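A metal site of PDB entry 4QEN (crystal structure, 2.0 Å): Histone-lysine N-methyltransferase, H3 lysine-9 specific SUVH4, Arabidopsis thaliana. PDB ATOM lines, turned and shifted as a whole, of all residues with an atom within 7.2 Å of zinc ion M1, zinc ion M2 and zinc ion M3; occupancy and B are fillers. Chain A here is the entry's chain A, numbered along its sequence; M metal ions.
Within 4 Å of zinc ion M1: Cys 292, Cys 306, Cys 334 and Cys 338.
The backbone NH of Cys 306 sits close to the side-chain sulfur of Cys 304 (3.4 Å).
N of Cys 340 sits at hydrogen-bond distance from O of Cys 294.
O of Cys 340 sits at hydrogen-bond distance from NH2 of Arg 347.
The backbone NH of Gly 339 sits at hydrogen-bond distance from the backbone carbonyl oxygen of Cys 292, 3.1 Å away.
The backbone NH (N) of Cys 334 sits at hydrogen-bond distance from the backbone carbonyl oxygen (O) of Asn 346, at 3.0 Å.
The side-chain sulfur (SG) of Cys 304 lies close to the backbone NH (N) of Ala 307 (3.4 Å).
SG of Cys 344 sits close to N of Asn 346.
N of Gly 335 lies close to SG of Cys 338 (3.2 Å).
Zinc ion M1 is bound by the side-chain sulfur of Cys 306 (2.3 Å), the side-chain sulfur of Cys 292 (2.3 Å), the side-chain sulfur of Cys 334 (2.4 Å) and the side-chain sulfur of Cys 338 (2.5 Å).
SG of Cys 340 binds zinc ion M2 (2.3 Å).
The side-chain sulfur (SG) of Cys 334 is bound to zinc ion M2 (2.3 Å).
Zinc ion M2 is bound by SG of Cys 344 (2.4 Å).
Zinc ion M2 is bound by the side-chain sulfur (SG) of Cys 298, 2.4 Å away.
Within 4 Å of zinc ion M2: Cys 298, Cys 334, Cys 340 and Cys 344.
The nearest printed residue that does not touch zinc ion M2 is Cys 292 (4.3 Å).
SG of Cys 298 binds zinc ion M3, at 2.3 Å.
SG of Cys 304 is bound to zinc ion M3, 2.4 Å away.
Zinc ion M3 is bound by SG of Cys 294 (2.4 Å).
SG of Cys 292 is bound to zinc ion M3, 2.4 Å away.
Zinc ion M3 has four donor atoms within binding distance.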
ATOM      1  N   THR A 290     -18.658  19.945  -0.396  1.00  0.00           N
ATOM      2  CA  THR A 290     -18.368  20.893   0.662  1.00  0.00           C
ATOM      3  C   THR A 290     -19.186  22.186   0.531  1.00  0.00           C
ATOM      4  O   THR A 290     -19.722  22.701   1.512  1.00  0.00           O
ATOM      5  CB  THR A 290     -16.865  21.221   0.707  1.00  0.00           C
ATOM      6  OG1 THR A 290     -16.125  20.018   0.938  1.00  0.00           O
ATOM      7  CG2 THR A 290     -16.566  22.222   1.799  1.00  0.00           C
ATOM      8  N   GLY A 291     -19.277  22.722  -0.685  1.00  0.00           N
ATOM      9  CA  GLY A 291     -20.061  23.928  -0.903  1.00  0.00           C
ATOM     10  C   GLY A 291     -19.359  25.239  -0.546  1.00  0.00           C
ATOM     11  O   GLY A 291     -18.204  25.264  -0.134  1.00  0.00           O
ATOM     12  N   CYS A 292     -20.097  26.342  -0.698  1.00  0.00           N
ATOM     13  CA  CYS A 292     -19.523  27.674  -0.522  1.00  0.00           C
ATOM     14  C   CYS A 292     -20.084  28.300   0.749  1.00  0.00           C
ATOM     15  O   CYS A 292     -21.047  27.779   1.327  1.00  0.00           O
ATOM     16  CB  CYS A 292     -19.882  28.558  -1.730  1.00  0.00           C
ATOM     17  SG  CYS A 292     -21.663  28.872  -1.923  1.00  0.00           S
ATOM     18  N   ASN A 293     -19.514  29.415   1.172  1.00  0.00           N
ATOM     19  CA  ASN A 293     -19.929  30.026   2.433  1.00  0.00           C
ATOM     20  C   ASN A 293     -20.679  31.328   2.228  1.00  0.00           C
ATOM     21  O   ASN A 293     -20.862  32.102   3.171  1.00  0.00           O
ATOM     22  CB  ASN A 293     -18.735  30.214   3.389  1.00  0.00           C
ATOM     23  CG  ASN A 293     -17.655  31.122   2.814  1.00  0.00           C
ATOM     24  OD1 ASN A 293     -17.883  31.873   1.869  1.00  0.00           O
ATOM     25  ND2 ASN A 293     -16.459  31.052   3.399  1.00  0.00           N
ATOM     26  N   CYS A 294     -21.079  31.574   0.981  1.00  0.00           N
ATOM     27  CA  CYS A 294     -21.811  32.776   0.646  1.00  0.00           C
ATOM     28  C   CYS A 294     -23.129  32.787   1.402  1.00  0.00           C
ATOM     29  O   CYS A 294     -23.617  31.741   1.822  1.00  0.00           O
ATOM     30  CB  CYS A 294     -22.078  32.852  -0.865  1.00  0.00           C
ATOM     31  SG  CYS A 294     -20.591  32.669  -1.891  1.00  0.00           S
ATOM     32  N   ARG A 295     -23.704  33.966   1.571  1.00  0.00           N
ATOM     33  CA  ARG A 295     -24.940  34.083   2.315  1.00  0.00           C
ATOM     34  C   ARG A 295     -26.071  34.629   1.455  1.00  0.00           C
ATOM     35  O   ARG A 295     -25.932  35.668   0.820  1.00  0.00           O
ATOM     36  CB  ARG A 295     -24.737  34.960   3.545  1.00  0.00           C
ATOM     37  CG  ARG A 295     -25.717  34.691   4.649  1.00  0.00           C
ATOM     38  CD  ARG A 295     -25.182  35.152   5.979  1.00  0.00           C
ATOM     39  NE  ARG A 295     -26.258  35.493   6.893  1.00  0.00           N
ATOM     40  CZ  ARG A 295     -26.976  34.606   7.568  1.00  0.00           C
ATOM     41  NH1 ARG A 295     -27.941  35.007   8.375  1.00  0.00           N
ATOM     42  NH2 ARG A 295     -26.715  33.313   7.435  1.00  0.00           N
ATOM     43  N   GLY A 296     -27.190  33.912   1.433  1.00  0.00           N
ATOM     44  CA  GLY A 296     -28.353  34.362   0.687  1.00  0.00           C
ATOM     45  C   GLY A 296     -28.308  33.965  -0.768  1.00  0.00           C
ATOM     46  O   GLY A 296     -28.977  33.010  -1.159  1.00  0.00           O
ATOM     47  N   SER A 297     -27.553  34.706  -1.564  1.00  0.00           N
ATOM     48  CA  SER A 297     -27.369  34.397  -2.986  1.00  0.00           C
ATOM     49  C   SER A 297     -25.909  34.547  -3.348  1.00  0.00           C
ATOM     50  O   SER A 297     -25.238  35.452  -2.853  1.00  0.00           O
ATOM     51  CB  SER A 297     -28.198  35.333  -3.859  1.00  0.00           C
ATOM     52  OG  SER A 297     -29.571  34.977  -3.859  1.00  0.00           O
ATOM     53  N   CYS A 298     -25.406  33.698  -4.227  1.00  0.00           N
ATOM     54  CA  CYS A 298     -24.006  33.822  -4.631  1.00  0.00           C
ATOM     55  C   CYS A 298     -23.835  34.808  -5.790  1.00  0.00           C
ATOM     56  O   CYS A 298     -24.401  34.612  -6.861  1.00  0.00           O
ATOM     57  CB  CYS A 298     -23.430  32.457  -4.983  1.00  0.00           C
ATOM     58  SG  CYS A 298     -23.581  31.355  -3.600  1.00  0.00           S
ATOM     59  N   THR A 299     -23.074  35.878  -5.540  1.00  0.00           N
ATOM     60  CA  THR A 299     -22.900  36.935  -6.548  1.00  0.00           C
ATOM     61  C   THR A 299     -21.443  37.344  -6.762  1.00  0.00           C
ATOM     62  O   THR A 299     -21.089  37.885  -7.812  1.00  0.00           O
ATOM     63  CB  THR A 299     -23.710  38.201  -6.208  1.00  0.00           C
ATOM     64  OG1 THR A 299     -23.495  38.534  -4.832  1.00  0.00           O
ATOM     65  CG2 THR A 299     -25.198  37.959  -6.440  1.00  0.00           C
ATOM     66  N   ASP A 300     -20.599  37.097  -5.769  1.00  0.00           N
ATOM     67  CA  ASP A 300     -19.187  37.419  -5.882  1.00  0.00           C
ATOM     68  C   ASP A 300     -18.404  36.169  -6.263  1.00  0.00           C
ATOM     69  O   ASP A 300     -18.212  35.264  -5.454  1.00  0.00           O
ATOM     70  CB  ASP A 300     -18.675  38.012  -4.568  1.00  0.00           C
ATOM     71  CG  ASP A 300     -17.262  38.554  -4.682  1.00  0.00           C
ATOM     72  OD1 ASP A 300     -16.393  37.868  -5.255  1.00  0.00           O
ATOM     73  OD2 ASP A 300     -17.019  39.689  -4.200  1.00  0.00           O
ATOM     74  N   LYS A 303     -15.261  35.166  -4.037  1.00  0.00           N
ATOM     75  CA  LYS A 303     -15.445  34.597  -2.708  1.00  0.00           C
ATOM     76  C   LYS A 303     -16.119  33.222  -2.741  1.00  0.00           C
ATOM     77  O   LYS A 303     -16.053  32.484  -1.759  1.00  0.00           O
ATOM     78  CB  LYS A 303     -16.264  35.551  -1.824  1.00  0.00           C
ATOM     79  CG  LYS A 303     -15.694  36.959  -1.728  1.00  0.00           C
ATOM     80  CD  LYS A 303     -16.249  37.680  -0.500  1.00  0.00           C
ATOM     81  CE  LYS A 303     -16.540  39.153  -0.787  1.00  0.00           C
ATOM     82  NZ  LYS A 303     -17.726  39.305  -1.702  1.00  0.00           N
ATOM     83  N   CYS A 304     -16.763  32.903  -3.851  1.00  0.00           N
ATOM     84  CA  CYS A 304     -17.601  31.704  -3.971  1.00  0.00           C
ATOM     85  C   CYS A 304     -16.862  30.480  -4.496  1.00  0.00           C
ATOM     86  O   CYS A 304     -16.462  30.439  -5.655  1.00  0.00           O
ATOM     87  CB  CYS A 304     -18.796  31.995  -4.877  1.00  0.00           C
ATOM     88  SG  CYS A 304     -19.903  30.562  -5.132  1.00  0.00           S
ATOM     89  N   ALA A 305     -16.704  29.470  -3.643  1.00  0.00           N
ATOM     90  CA  ALA A 305     -16.044  28.220  -4.033  1.00  0.00           C
ATOM     91  C   ALA A 305     -16.731  27.519  -5.215  1.00  0.00           C
ATOM     92  O   ALA A 305     -16.093  26.793  -5.998  1.00  0.00           O
ATOM     93  CB  ALA A 305     -15.963  27.277  -2.827  1.00  0.00           C
ATOM     94  N   CYS A 306     -18.029  27.745  -5.351  1.00  0.00           N
ATOM     95  CA  CYS A 306     -18.805  27.104  -6.400  1.00  0.00           C
ATOM     96  C   CYS A 306     -18.568  27.786  -7.753  1.00  0.00           C
ATOM     97  O   CYS A 306     -18.559  27.124  -8.791  1.00  0.00           O
ATOM     98  CB  CYS A 306     -20.288  27.063  -6.025  1.00  0.00           C
ATOM     99  SG  CYS A 306     -20.646  26.133  -4.479  1.00  0.00           S
ATOM    100  N   ALA A 307     -18.347  29.092  -7.739  1.00  0.00           N
ATOM    101  CA  ALA A 307     -17.914  29.794  -8.945  1.00  0.00           C
ATOM    102  C   ALA A 307     -16.512  29.316  -9.320  1.00  0.00           C
ATOM    103  O   ALA A 307     -16.199  29.161 -10.502  1.00  0.00           O
ATOM    104  CB  ALA A 307     -17.926  31.314  -8.725  1.00  0.00           C
ATOM    105  N   PHE A 314     -19.666  32.428 -12.863  1.00  0.00           N
ATOM    106  CA  PHE A 314     -20.916  31.689 -12.759  1.00  0.00           C
ATOM    107  C   PHE A 314     -21.350  31.239 -14.146  1.00  0.00           C
ATOM    108  O   PHE A 314     -21.212  31.985 -15.111  1.00  0.00           O
ATOM    109  CB  PHE A 314     -21.980  32.552 -12.080  1.00  0.00           C
ATOM    110  CG  PHE A 314     -21.687  32.819 -10.623  1.00  0.00           C
ATOM    111  CD1 PHE A 314     -21.936  31.849  -9.666  1.00  0.00           C
ATOM    112  CD2 PHE A 314     -21.150  34.027 -10.223  1.00  0.00           C
ATOM    113  CE1 PHE A 314     -21.653  32.092  -8.316  1.00  0.00           C
ATOM    114  CE2 PHE A 314     -20.879  34.279  -8.885  1.00  0.00           C
ATOM    115  CZ  PHE A 314     -21.124  33.300  -7.938  1.00  0.00           C
ATOM    116  N   PHE A 332     -21.218  23.195 -12.181  1.00  0.00           N
ATOM    117  CA  PHE A 332     -21.212  22.983 -10.734  1.00  0.00           C
ATOM    118  C   PHE A 332     -22.167  23.939 -10.038  1.00  0.00           C
ATOM    119  O   PHE A 332     -21.900  25.143  -9.957  1.00  0.00           O
ATOM    120  CB  PHE A 332     -19.805  23.162 -10.170  1.00  0.00           C
ATOM    121  CG  PHE A 332     -18.818  22.138 -10.662  1.00  0.00           C
ATOM    122  CD1 PHE A 332     -18.619  20.961  -9.968  1.00  0.00           C
ATOM    123  CD2 PHE A 332     -18.079  22.372 -11.817  1.00  0.00           C
ATOM    124  CE1 PHE A 332     -17.701  20.023 -10.420  1.00  0.00           C
ATOM    125  CE2 PHE A 332     -17.163  21.448 -12.273  1.00  0.00           C
ATOM    126  CZ  PHE A 332     -16.971  20.271 -11.572  1.00  0.00           C
ATOM    127  N   GLU A 333     -23.283  23.417  -9.553  1.00  0.00           N
ATOM    128  CA  GLU A 333     -24.287  24.220  -8.852  1.00  0.00           C
ATOM    129  C   GLU A 333     -24.064  24.201  -7.347  1.00  0.00           C
ATOM    130  O   GLU A 333     -23.439  23.279  -6.828  1.00  0.00           O
ATOM    131  CB  GLU A 333     -25.697  23.717  -9.159  1.00  0.00           C
ATOM    132  CG  GLU A 333     -26.263  24.241 -10.489  1.00  0.00           C
ATOM    133  CD  GLU A 333     -27.672  23.737 -10.766  1.00  0.00           C
ATOM    134  OE1 GLU A 333     -28.236  22.972  -9.950  1.00  0.00           O
ATOM    135  OE2 GLU A 333     -28.211  24.113 -11.822  1.00  0.00           O
ATOM    136  N   CYS A 334     -24.589  25.210  -6.655  1.00  0.00           N
ATOM    137  CA  CYS A 334     -24.608  25.211  -5.191  1.00  0.00           C
ATOM    138  C   CYS A 334     -25.477  24.036  -4.713  1.00  0.00           C
ATOM    139  O   CYS A 334     -26.340  23.556  -5.467  1.00  0.00           O
ATOM    140  CB  CYS A 334     -25.114  26.547  -4.657  1.00  0.00           C
ATOM    141  SG  CYS A 334     -23.988  27.911  -5.022  1.00  0.00           S
ATOM    142  N   GLY A 335     -25.233  23.569  -3.492  1.00  0.00           N
ATOM    143  CA  GLY A 335     -25.878  22.359  -3.003  1.00  0.00           C
ATOM    144  C   GLY A 335     -26.240  22.417  -1.529  1.00  0.00           C
ATOM    145  O   GLY A 335     -26.297  23.499  -0.944  1.00  0.00           O
ATOM    146  N   HIS A 337     -24.935  21.974   1.286  1.00  0.00           N
ATOM    147  CA  HIS A 337     -24.091  22.579   2.320  1.00  0.00           C
ATOM    148  C   HIS A 337     -23.693  24.012   2.024  1.00  0.00           C
ATOM    149  O   HIS A 337     -22.957  24.623   2.798  1.00  0.00           O
ATOM    150  CB  HIS A 337     -22.851  21.719   2.582  1.00  0.00           C
ATOM    151  CG  HIS A 337     -23.162  20.402   3.208  1.00  0.00           C
ATOM    152  ND1 HIS A 337     -23.761  20.287   4.435  1.00  0.00           N
ATOM    153  CD2 HIS A 337     -22.959  19.133   2.765  1.00  0.00           C
ATOM    154  CE1 HIS A 337     -23.924  19.010   4.741  1.00  0.00           C
ATOM    155  NE2 HIS A 337     -23.440  18.284   3.738  1.00  0.00           N
ATOM    156  N   CYS A 338     -24.166  24.555   0.909  1.00  0.00           N
ATOM    157  CA  CYS A 338     -23.851  25.954   0.618  1.00  0.00           C
ATOM    158  C   CYS A 338     -24.613  26.868   1.575  1.00  0.00           C
ATOM    159  O   CYS A 338     -25.688  26.517   2.046  1.00  0.00           O
ATOM    160  CB  CYS A 338     -24.168  26.285  -0.834  1.00  0.00           C
ATOM    161  SG  CYS A 338     -23.110  25.377  -1.977  1.00  0.00           S
ATOM    162  N   GLY A 339     -24.057  28.029   1.856  1.00  0.00           N
ATOM    163  CA  GLY A 339     -24.715  28.980   2.743  1.00  0.00           C
ATOM    164  C   GLY A 339     -25.848  29.745   2.075  1.00  0.00           C
ATOM    165  O   GLY A 339     -26.595  30.466   2.752  1.00  0.00           O
ATOM    166  N   CYS A 340     -25.995  29.600   0.767  1.00  0.00           N
ATOM    167  CA  CYS A 340     -27.001  30.346   0.027  1.00  0.00           C
ATOM    168  C   CYS A 340     -28.342  29.629   0.027  1.00  0.00           C
ATOM    169  O   CYS A 340     -28.403  28.417   0.190  1.00  0.00           O
ATOM    170  CB  CYS A 340     -26.557  30.533  -1.426  1.00  0.00           C
ATOM    171  SG  CYS A 340     -26.314  28.950  -2.256  1.00  0.00           S
ATOM    172  N   GLY A 341     -29.408  30.399  -0.170  1.00  0.00           N
ATOM    173  CA  GLY A 341     -30.759  29.866  -0.221  1.00  0.00           C
ATOM    174  C   GLY A 341     -31.197  29.560  -1.649  1.00  0.00           C
ATOM    175  O   GLY A 341     -30.424  29.750  -2.600  1.00  0.00           O
ATOM    176  N   LYS A 343     -32.941  30.890  -3.890  1.00  0.00           N
ATOM    177  CA  LYS A 343     -33.002  31.925  -4.929  1.00  0.00           C
ATOM    178  C   LYS A 343     -31.684  32.093  -5.669  1.00  0.00           C
ATOM    179  O   LYS A 343     -31.648  32.722  -6.726  1.00  0.00           O
ATOM    180  CB  LYS A 343     -33.430  33.273  -4.333  1.00  0.00           C
ATOM    181  CG  LYS A 343     -34.904  33.366  -3.988  1.00  0.00           C
ATOM    182  CD  LYS A 343     -35.282  34.797  -3.615  1.00  0.00           C
ATOM    183  CE  LYS A 343     -36.748  34.898  -3.206  1.00  0.00           C
ATOM    184  NZ  LYS A 343     -37.092  36.262  -2.726  1.00  0.00           N
ATOM    185  N   CYS A 344     -30.608  31.527  -5.125  1.00  0.00           N
ATOM    186  CA  CYS A 344     -29.287  31.626  -5.746  1.00  0.00           C
ATOM    187  C   CYS A 344     -29.290  31.287  -7.237  1.00  0.00           C
ATOM    188  O   CYS A 344     -29.868  30.281  -7.662  1.00  0.00           O
ATOM    189  CB  CYS A 344     -28.277  30.727  -5.035  1.00  0.00           C
ATOM    190  SG  CYS A 344     -26.649  30.862  -5.749  1.00  0.00           S
ATOM    191  N   VAL A 345     -28.654  32.127  -8.030  1.00  0.00           N
ATOM    192  CA  VAL A 345     -28.668  31.919  -9.485  1.00  0.00           C
ATOM    193  C   VAL A 345     -27.852  30.670  -9.848  1.00  0.00           C
ATOM    194  O   VAL A 345     -28.146  29.973 -10.829  1.00  0.00           O
ATOM    195  CB  VAL A 345     -28.167  33.164 -10.241  1.00  0.00           C
ATOM    196  CG1 VAL A 345     -28.183  32.943 -11.753  1.00  0.00           C
ATOM    197  CG2 VAL A 345     -29.067  34.361  -9.887  1.00  0.00           C
ATOM    198  N   ASN A 346     -26.877  30.342  -9.014  1.00  0.00           N
ATOM    199  CA  ASN A 346     -26.124  29.115  -9.203  1.00  0.00           C
ATOM    200  C   ASN A 346     -26.885  27.878  -8.686  1.00  0.00           C
ATOM    201  O   ASN A 346     -26.291  26.826  -8.468  1.00  0.00           O
ATOM    202  CB  ASN A 346     -24.731  29.231  -8.578  1.00  0.00           C
ATOM    203  CG  ASN A 346     -23.723  28.324  -9.254  1.00  0.00           C
ATOM    204  OD1 ASN A 346     -23.726  28.194 -10.465  1.00  0.00           O
ATOM    205  ND2 ASN A 346     -22.866  27.669  -8.456  1.00  0.00           N
ATOM    206  N   ARG A 347     -28.187  28.004  -8.482  1.00  0.00           N
ATOM    207  CA  ARG A 347     -29.053  26.849  -8.312  1.00  0.00           C
ATOM    208  C   ARG A 347     -30.130  26.850  -9.390  1.00  0.00           C
ATOM    209  O   ARG A 347     -31.233  26.333  -9.186  1.00  0.00           O
ATOM    210  CB  ARG A 347     -29.747  26.853  -6.946  1.00  0.00           C
ATOM    211  CG  ARG A 347     -28.811  26.790  -5.749  1.00  0.00           C
ATOM    212  CD  ARG A 347     -29.612  26.955  -4.472  1.00  0.00           C
ATOM    213  NE  ARG A 347     -28.792  26.964  -3.266  1.00  0.00           N
ATOM    214  CZ  ARG A 347     -28.466  25.858  -2.606  1.00  0.00           C
ATOM    215  NH1 ARG A 347     -28.884  24.687  -3.061  1.00  0.00           N
ATOM    216  NH2 ARG A 347     -27.734  25.928  -1.491  1.00  0.00           N
HETATM  217 ZN    ZN M   1     -22.322  27.197  -3.417  1.00  0.00          ZN
HETATM  218 ZN    ZN M   2     -25.260  29.694  -4.175  1.00  0.00          ZN
HETATM  219 ZN    ZN M   3     -21.363  30.850  -3.262  1.00  0.00          ZN
